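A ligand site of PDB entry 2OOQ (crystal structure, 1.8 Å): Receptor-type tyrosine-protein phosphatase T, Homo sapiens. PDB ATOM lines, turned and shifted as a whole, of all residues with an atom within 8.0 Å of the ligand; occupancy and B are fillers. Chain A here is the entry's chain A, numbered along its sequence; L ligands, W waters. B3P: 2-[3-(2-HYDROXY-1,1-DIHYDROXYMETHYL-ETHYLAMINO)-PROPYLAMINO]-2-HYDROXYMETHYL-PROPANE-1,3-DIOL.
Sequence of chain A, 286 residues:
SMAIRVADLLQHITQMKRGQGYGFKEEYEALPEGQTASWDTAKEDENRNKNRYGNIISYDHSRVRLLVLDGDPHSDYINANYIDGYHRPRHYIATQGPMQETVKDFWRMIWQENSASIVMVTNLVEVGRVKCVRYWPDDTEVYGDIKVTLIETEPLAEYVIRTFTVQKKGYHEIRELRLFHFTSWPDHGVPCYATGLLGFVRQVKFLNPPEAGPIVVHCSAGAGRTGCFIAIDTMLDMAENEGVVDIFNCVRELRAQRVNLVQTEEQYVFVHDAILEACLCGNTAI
A nitrogen (N1) of the ligand is in salt-bridge range of the side-chain carboxylate (OE1) of Glu 154 (3.996 Å).
O5 of the ligand sits at hydrogen-bond distance from OG1 of Thr 163, at 2.6 Å.
The guanidinium group of Arg 178 lies within hydrogen-bond range of an oxygen (O5) of the ligand (2.9 Å).
A nitrogen (N1) of the ligand is in salt-bridge range of the side-chain carboxylate (OE2) of Glu 152 (3.1 Å).
The backbone NH of Glu 154 sits at hydrogen-bond distance from the backbone carbonyl oxygen of Ile 161, 2.7 Å away.
The backbone NH of Thr 163 lies within hydrogen-bond range of the backbone carbonyl oxygen of Glu 152, at 2.9 Å.
The backbone carbonyl oxygen of Thr 163 is in hydrogen-bond range of the backbone NH of Ile 151 (2.9 Å).
The guanidinium group of Arg 178 lies within hydrogen-bond range of the backbone carbonyl oxygen of Leu 207.
The guanidinium group (NH2) of Arg 178 lies within salt-bridge range of the side-chain carboxylate (OE1) of Glu 176 (3.5 Å).
CG2 of Ile 161 touches O6 of the ligand, 3.9 Å away.
Leu 207 touches the ligand.
Hydrophobic or aromatic side chains within 4 Å of the ligand: Ile 161 and Leu 207.
The nearest printed residue that does not touch the ligand is Glu 176 (5.1 Å).
Water W3 bridges N1 of the ligand (2.9 Å) and OE1 of Glu 152 (2.9 Å).
Water W2 lies within hydrogen-bond range of OG1 of Thr 163 (2.8 Å), O of Ile 161 (2.8 Å), O6 of the ligand (2.9 Å) and O of Glu 152 (3.3 Å).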
ATOM      1  N   ILE A 151       4.725 -31.694  -5.301  1.00  0.00           N
ATOM      2  CA  ILE A 151       3.644 -32.682  -5.143  1.00  0.00           C
ATOM      3  C   ILE A 151       2.352 -32.389  -5.906  1.00  0.00           C
ATOM      4  O   ILE A 151       1.528 -33.277  -6.076  1.00  0.00           O
ATOM      5  CB  ILE A 151       3.351 -32.991  -3.637  1.00  0.00           C
ATOM      6  CG1 ILE A 151       2.735 -31.780  -2.932  1.00  0.00           C
ATOM      7  CG2 ILE A 151       4.654 -33.544  -2.929  1.00  0.00           C
ATOM      8  CD1 ILE A 151       2.238 -32.076  -1.481  1.00  0.00           C
ATOM      9  N   GLU A 152       2.138 -31.160  -6.360  1.00  0.00           N
ATOM     10  CA  GLU A 152       0.954 -30.844  -7.175  1.00  0.00           C
ATOM     11  C   GLU A 152       1.171 -29.591  -8.008  1.00  0.00           C
ATOM     12  O   GLU A 152       1.816 -28.636  -7.539  1.00  0.00           O
ATOM     13  CB  GLU A 152      -0.299 -30.681  -6.296  1.00  0.00           C
ATOM     14  CG  GLU A 152      -1.610 -30.539  -7.080  1.00  0.00           C
ATOM     15  CD  GLU A 152      -2.848 -30.361  -6.160  1.00  0.00           C
ATOM     16  OE1 GLU A 152      -2.842 -30.778  -4.984  1.00  0.00           O
ATOM     17  OE2 GLU A 152      -3.851 -29.800  -6.622  1.00  0.00           O
ATOM     18  N   THR A 153       0.659 -29.606  -9.234  1.00  0.00           N
ATOM     19  CA  THR A 153       0.592 -28.353 -10.065  1.00  0.00           C
ATOM     20  C   THR A 153      -0.863 -28.120 -10.481  1.00  0.00           C
ATOM     21  O   THR A 153      -1.516 -29.018 -11.000  1.00  0.00           O
ATOM     22  CB  THR A 153       1.478 -28.458 -11.267  1.00  0.00           C
ATOM     23  OG1 THR A 153       2.804 -28.813 -10.865  1.00  0.00           O
ATOM     24  CG2 THR A 153       1.497 -27.133 -12.016  1.00  0.00           C
ATOM     25  N   GLU A 154      -1.386 -26.918 -10.216  1.00  0.00           N
ATOM     26  CA  GLU A 154      -2.749 -26.562 -10.583  1.00  0.00           C
ATOM     27  C   GLU A 154      -2.723 -25.338 -11.479  1.00  0.00           C
ATOM     28  O   GLU A 154      -2.618 -24.207 -10.998  1.00  0.00           O
ATOM     29  CB  GLU A 154      -3.621 -26.300  -9.329  1.00  0.00           C
ATOM     30  CG  GLU A 154      -5.109 -26.096  -9.659  1.00  0.00           C
ATOM     31  CD  GLU A 154      -5.941 -25.569  -8.501  1.00  0.00           C
ATOM     32  OE1 GLU A 154      -5.411 -25.341  -7.396  1.00  0.00           O
ATOM     33  OE2 GLU A 154      -7.167 -25.387  -8.696  1.00  0.00           O
ATOM     34  N   PRO A 155      -2.754 -25.553 -12.803  1.00  0.00           N
ATOM     35  CA  PRO A 155      -2.780 -24.433 -13.742  1.00  0.00           C
ATOM     36  C   PRO A 155      -4.148 -23.827 -13.928  1.00  0.00           C
ATOM     37  O   PRO A 155      -5.130 -24.542 -14.108  1.00  0.00           O
ATOM     38  CB  PRO A 155      -2.286 -25.062 -15.045  1.00  0.00           C
ATOM     39  CG  PRO A 155      -2.679 -26.490 -14.955  1.00  0.00           C
ATOM     40  CD  PRO A 155      -2.682 -26.854 -13.488  1.00  0.00           C
ATOM     41  N   LEU A 156      -4.201 -22.516 -13.902  1.00  0.00           N
ATOM     42  CA  LEU A 156      -5.427 -21.804 -14.160  1.00  0.00           C
ATOM     43  C   LEU A 156      -5.096 -20.778 -15.227  1.00  0.00           C
ATOM     44  O   LEU A 156      -3.940 -20.739 -15.718  1.00  0.00           O
ATOM     45  CB  LEU A 156      -5.924 -21.183 -12.864  1.00  0.00           C
ATOM     46  CG  LEU A 156      -6.568 -22.201 -11.920  1.00  0.00           C
ATOM     47  CD1 LEU A 156      -5.993 -22.120 -10.525  1.00  0.00           C
ATOM     48  CD2 LEU A 156      -8.085 -22.012 -11.897  1.00  0.00           C
ATOM     49  N   TYR A 159      -2.748 -17.759 -13.663  1.00  0.00           N
ATOM     50  CA  TYR A 159      -1.788 -18.144 -12.657  1.00  0.00           C
ATOM     51  C   TYR A 159      -1.767 -19.652 -12.476  1.00  0.00           C
ATOM     52  O   TYR A 159      -2.634 -20.348 -12.992  1.00  0.00           O
ATOM     53  CB  TYR A 159      -2.109 -17.452 -11.343  1.00  0.00           C
ATOM     54  CG  TYR A 159      -3.472 -17.805 -10.757  1.00  0.00           C
ATOM     55  CD1 TYR A 159      -3.602 -18.857  -9.865  1.00  0.00           C
ATOM     56  CD2 TYR A 159      -4.606 -17.073 -11.073  1.00  0.00           C
ATOM     57  CE1 TYR A 159      -4.809 -19.183  -9.315  1.00  0.00           C
ATOM     58  CE2 TYR A 159      -5.824 -17.407 -10.540  1.00  0.00           C
ATOM     59  CZ  TYR A 159      -5.917 -18.461  -9.649  1.00  0.00           C
ATOM     60  OH  TYR A 159      -7.096 -18.813  -9.065  1.00  0.00           O
ATOM     61  N   VAL A 160      -0.763 -20.116 -11.733  1.00  0.00           N
ATOM     62  CA  VAL A 160      -0.541 -21.552 -11.465  1.00  0.00           C
ATOM     63  C   VAL A 160      -0.134 -21.672 -10.000  1.00  0.00           C
ATOM     64  O   VAL A 160       0.718 -20.920  -9.510  1.00  0.00           O
ATOM     65  CB  VAL A 160       0.551 -22.205 -12.358  1.00  0.00           C
ATOM     66  CG1 VAL A 160       1.879 -21.466 -12.261  1.00  0.00           C
ATOM     67  CG2 VAL A 160       0.736 -23.734 -12.023  1.00  0.00           C
ATOM     68  N   ILE A 161      -0.751 -22.628  -9.314  1.00  0.00           N
ATOM     69  CA  ILE A 161      -0.364 -22.954  -7.937  1.00  0.00           C
ATOM     70  C   ILE A 161       0.377 -24.274  -7.924  1.00  0.00           C
ATOM     71  O   ILE A 161      -0.126 -25.312  -8.403  1.00  0.00           O
ATOM     72  CB  ILE A 161      -1.563 -23.085  -7.010  1.00  0.00           C
ATOM     73  CG1 ILE A 161      -2.442 -21.850  -7.145  1.00  0.00           C
ATOM     74  CG2 ILE A 161      -1.100 -23.292  -5.537  1.00  0.00           C
ATOM     75  CD1 ILE A 161      -3.800 -22.015  -6.408  1.00  0.00           C
ATOM     76  N   ARG A 162       1.590 -24.212  -7.403  1.00  0.00           N
ATOM     77  CA  ARG A 162       2.396 -25.387  -7.237  1.00  0.00           C
ATOM     78  C   ARG A 162       2.579 -25.657  -5.751  1.00  0.00           C
ATOM     79  O   ARG A 162       2.864 -24.736  -4.961  1.00  0.00           O
ATOM     80  CB  ARG A 162       3.749 -25.182  -7.885  1.00  0.00           C
ATOM     81  CG  ARG A 162       3.692 -25.032  -9.376  1.00  0.00           C
ATOM     82  CD  ARG A 162       5.090 -24.994  -9.961  1.00  0.00           C
ATOM     83  NE  ARG A 162       5.071 -24.684 -11.384  1.00  0.00           N
ATOM     84  CZ  ARG A 162       5.073 -23.469 -11.904  1.00  0.00           C
ATOM     85  NH1 ARG A 162       5.093 -22.373 -11.135  1.00  0.00           N
ATOM     86  NH2 ARG A 162       5.064 -23.339 -13.229  1.00  0.00           N
ATOM     87  N   THR A 163       2.403 -26.897  -5.357  1.00  0.00           N
ATOM     88  CA  THR A 163       2.489 -27.248  -3.954  1.00  0.00           C
ATOM     89  C   THR A 163       3.694 -28.166  -3.783  1.00  0.00           C
ATOM     90  O   THR A 163       3.905 -29.039  -4.616  1.00  0.00           O
ATOM     91  CB  THR A 163       1.212 -28.007  -3.503  1.00  0.00           C
ATOM     92  OG1 THR A 163       0.034 -27.218  -3.765  1.00  0.00           O
ATOM     93  CG2 THR A 163       1.227 -28.348  -2.024  1.00  0.00           C
ATOM     94  N   PHE A 164       4.447 -27.974  -2.704  1.00  0.00           N
ATOM     95  CA  PHE A 164       5.692 -28.711  -2.458  1.00  0.00           C
ATOM     96  C   PHE A 164       5.731 -29.211  -1.031  1.00  0.00           C
ATOM     97  O   PHE A 164       5.165 -28.585  -0.155  1.00  0.00           O
ATOM     98  CB  PHE A 164       6.940 -27.803  -2.592  1.00  0.00           C
ATOM     99  CG  PHE A 164       7.052 -27.117  -3.911  1.00  0.00           C
ATOM    100  CD1 PHE A 164       7.705 -27.727  -4.954  1.00  0.00           C
ATOM    101  CD2 PHE A 164       6.493 -25.847  -4.094  1.00  0.00           C
ATOM    102  CE1 PHE A 164       7.807 -27.122  -6.218  1.00  0.00           C
ATOM    103  CE2 PHE A 164       6.575 -25.217  -5.328  1.00  0.00           C
ATOM    104  CZ  PHE A 164       7.248 -25.852  -6.419  1.00  0.00           C
ATOM    105  N   GLU A 176       4.508 -28.174   4.227  1.00  0.00           N
ATOM    106  CA  GLU A 176       3.878 -28.008   2.928  1.00  0.00           C
ATOM    107  C   GLU A 176       3.962 -26.518   2.612  1.00  0.00           C
ATOM    108  O   GLU A 176       3.723 -25.680   3.485  1.00  0.00           O
ATOM    109  CB  GLU A 176       2.395 -28.452   2.986  1.00  0.00           C
ATOM    110  CG  GLU A 176       1.729 -28.459   1.618  1.00  0.00           C
ATOM    111  CD  GLU A 176       0.362 -29.078   1.612  1.00  0.00           C
ATOM    112  OE1 GLU A 176      -0.590 -28.475   2.191  1.00  0.00           O
ATOM    113  OE2 GLU A 176       0.245 -30.178   1.035  1.00  0.00           O
ATOM    114  N   LEU A 177       4.318 -26.204   1.382  1.00  0.00           N
ATOM    115  CA  LEU A 177       4.443 -24.825   0.912  1.00  0.00           C
ATOM    116  C   LEU A 177       3.744 -24.731  -0.430  1.00  0.00           C
ATOM    117  O   LEU A 177       3.826 -25.655  -1.247  1.00  0.00           O
ATOM    118  CB  LEU A 177       5.908 -24.439   0.782  1.00  0.00           C
ATOM    119  CG  LEU A 177       6.173 -23.019   0.271  1.00  0.00           C
ATOM    120  CD1 LEU A 177       7.300 -22.321   1.062  1.00  0.00           C
ATOM    121  CD2 LEU A 177       6.442 -23.042  -1.217  1.00  0.00           C
ATOM    122  N   ARG A 178       3.073 -23.616  -0.663  1.00  0.00           N
ATOM    123  CA  ARG A 178       2.512 -23.306  -1.976  1.00  0.00           C
ATOM    124  C   ARG A 178       3.143 -22.101  -2.590  1.00  0.00           C
ATOM    125  O   ARG A 178       3.352 -21.064  -1.917  1.00  0.00           O
ATOM    126  CB  ARG A 178       1.002 -23.070  -1.849  1.00  0.00           C
ATOM    127  CG  ARG A 178       0.227 -24.282  -1.349  1.00  0.00           C
ATOM    128  CD  ARG A 178      -1.251 -23.938  -1.137  1.00  0.00           C
ATOM    129  NE  ARG A 178      -1.979 -25.062  -0.536  1.00  0.00           N
ATOM    130  CZ  ARG A 178      -2.411 -25.101   0.715  1.00  0.00           C
ATOM    131  NH1 ARG A 178      -2.228 -24.080   1.538  1.00  0.00           N
ATOM    132  NH2 ARG A 178      -3.052 -26.172   1.137  1.00  0.00           N
ATOM    133  N   LEU A 179       3.464 -22.231  -3.875  1.00  0.00           N
ATOM    134  CA  LEU A 179       3.919 -21.141  -4.722  1.00  0.00           C
ATOM    135  C   LEU A 179       2.793 -20.701  -5.637  1.00  0.00           C
ATOM    136  O   LEU A 179       2.311 -21.466  -6.495  1.00  0.00           O
ATOM    137  CB  LEU A 179       5.160 -21.594  -5.506  1.00  0.00           C
ATOM    138  CG  LEU A 179       5.689 -20.782  -6.687  1.00  0.00           C
ATOM    139  CD1 LEU A 179       5.818 -19.295  -6.339  1.00  0.00           C
ATOM    140  CD2 LEU A 179       7.042 -21.403  -7.161  1.00  0.00           C
ATOM    141  N   PHE A 180       2.284 -19.504  -5.356  1.00  0.00           N
ATOM    142  CA  PHE A 180       1.245 -18.901  -6.134  1.00  0.00           C
ATOM    143  C   PHE A 180       1.935 -18.059  -7.205  1.00  0.00           C
ATOM    144  O   PHE A 180       2.534 -17.039  -6.924  1.00  0.00           O
ATOM    145  CB  PHE A 180       0.360 -18.030  -5.218  1.00  0.00           C
ATOM    146  CG  PHE A 180      -0.336 -18.795  -4.138  1.00  0.00           C
ATOM    147  CD1 PHE A 180      -1.592 -19.322  -4.350  1.00  0.00           C
ATOM    148  CD2 PHE A 180       0.256 -18.992  -2.897  1.00  0.00           C
ATOM    149  CE1 PHE A 180      -2.258 -20.031  -3.355  1.00  0.00           C
ATOM    150  CE2 PHE A 180      -0.421 -19.710  -1.885  1.00  0.00           C
ATOM    151  CZ  PHE A 180      -1.658 -20.226  -2.120  1.00  0.00           C
ATOM    152  N   GLN A 203      -7.402 -16.772  -3.744  1.00  0.00           N
ATOM    153  CA  GLN A 203      -6.765 -18.079  -3.458  1.00  0.00           C
ATOM    154  C   GLN A 203      -5.746 -18.041  -2.318  1.00  0.00           C
ATOM    155  O   GLN A 203      -5.714 -18.943  -1.464  1.00  0.00           O
ATOM    156  CB  GLN A 203      -6.036 -18.608  -4.708  1.00  0.00           C
ATOM    157  CG  GLN A 203      -6.950 -18.925  -5.864  1.00  0.00           C
ATOM    158  CD  GLN A 203      -7.296 -20.412  -5.978  1.00  0.00           C
ATOM    159  OE1 GLN A 203      -7.291 -21.129  -4.985  1.00  0.00           O
ATOM    160  NE2 GLN A 203      -7.636 -20.855  -7.191  1.00  0.00           N
ATOM    161  N   PHE A 206      -7.516 -17.602   0.944  1.00  0.00           N
ATOM    162  CA  PHE A 206      -8.192 -18.860   1.297  1.00  0.00           C
ATOM    163  C   PHE A 206      -7.220 -19.932   1.766  1.00  0.00           C
ATOM    164  O   PHE A 206      -7.489 -20.660   2.704  1.00  0.00           O
ATOM    165  CB  PHE A 206      -8.928 -19.424   0.079  1.00  0.00           C
ATOM    166  CG  PHE A 206      -9.822 -20.580   0.409  1.00  0.00           C
ATOM    167  CD1 PHE A 206     -11.059 -20.362   0.995  1.00  0.00           C
ATOM    168  CD2 PHE A 206      -9.443 -21.884   0.097  1.00  0.00           C
ATOM    169  CE1 PHE A 206     -11.895 -21.432   1.304  1.00  0.00           C
ATOM    170  CE2 PHE A 206     -10.271 -22.953   0.400  1.00  0.00           C
ATOM    171  CZ  PHE A 206     -11.495 -22.741   1.003  1.00  0.00           C
ATOM    172  N   LEU A 207      -6.095 -20.046   1.081  1.00  0.00           N
ATOM    173  CA  LEU A 207      -5.227 -21.221   1.281  1.00  0.00           C
ATOM    174  C   LEU A 207      -4.068 -21.003   2.241  1.00  0.00           C
ATOM    175  O   LEU A 207      -3.562 -21.965   2.811  1.00  0.00           O
ATOM    176  CB  LEU A 207      -4.706 -21.709  -0.075  1.00  0.00           C
ATOM    177  CG  LEU A 207      -5.714 -22.388  -1.005  1.00  0.00           C
ATOM    178  CD1 LEU A 207      -5.111 -22.702  -2.350  1.00  0.00           C
ATOM    179  CD2 LEU A 207      -6.252 -23.681  -0.366  1.00  0.00           C
HETATM  180  C1  B3P L   1      -7.100 -28.524  -6.142  1.00  0.00           C
HETATM  181  C2  B3P L   1      -8.444 -28.108  -6.727  1.00  0.00           C
HETATM  182  C3  B3P L   1      -6.579 -27.533  -5.064  1.00  0.00           C
HETATM  183  N1  B3P L   1      -5.337 -28.062  -4.470  1.00  0.00           N
HETATM  184  C4  B3P L   1      -4.423 -27.139  -3.739  1.00  0.00           C
HETATM  185  C5  B3P L   1      -5.063 -26.657  -2.428  1.00  0.00           C
HETATM  186  C6  B3P L   1      -3.092 -27.896  -3.431  1.00  0.00           C
HETATM  187  C7  B3P L   1      -4.087 -25.914  -4.569  1.00  0.00           C
HETATM  188  O4  B3P L   1      -5.527 -27.747  -1.644  1.00  0.00           O
HETATM  189  O5  B3P L   1      -2.255 -27.203  -2.510  1.00  0.00           O
HETATM  190  O6  B3P L   1      -3.660 -26.243  -5.901  1.00  0.00           O
HETATM  191  O   HOH W   1      -8.384 -25.082  -4.080  1.00  0.00           O
HETATM  192  O   HOH W   2      -0.930 -27.113  -6.397  1.00  0.00           O
HETATM  193  O   HOH W   3      -5.243 -30.706  -3.321  1.00  0.00           O
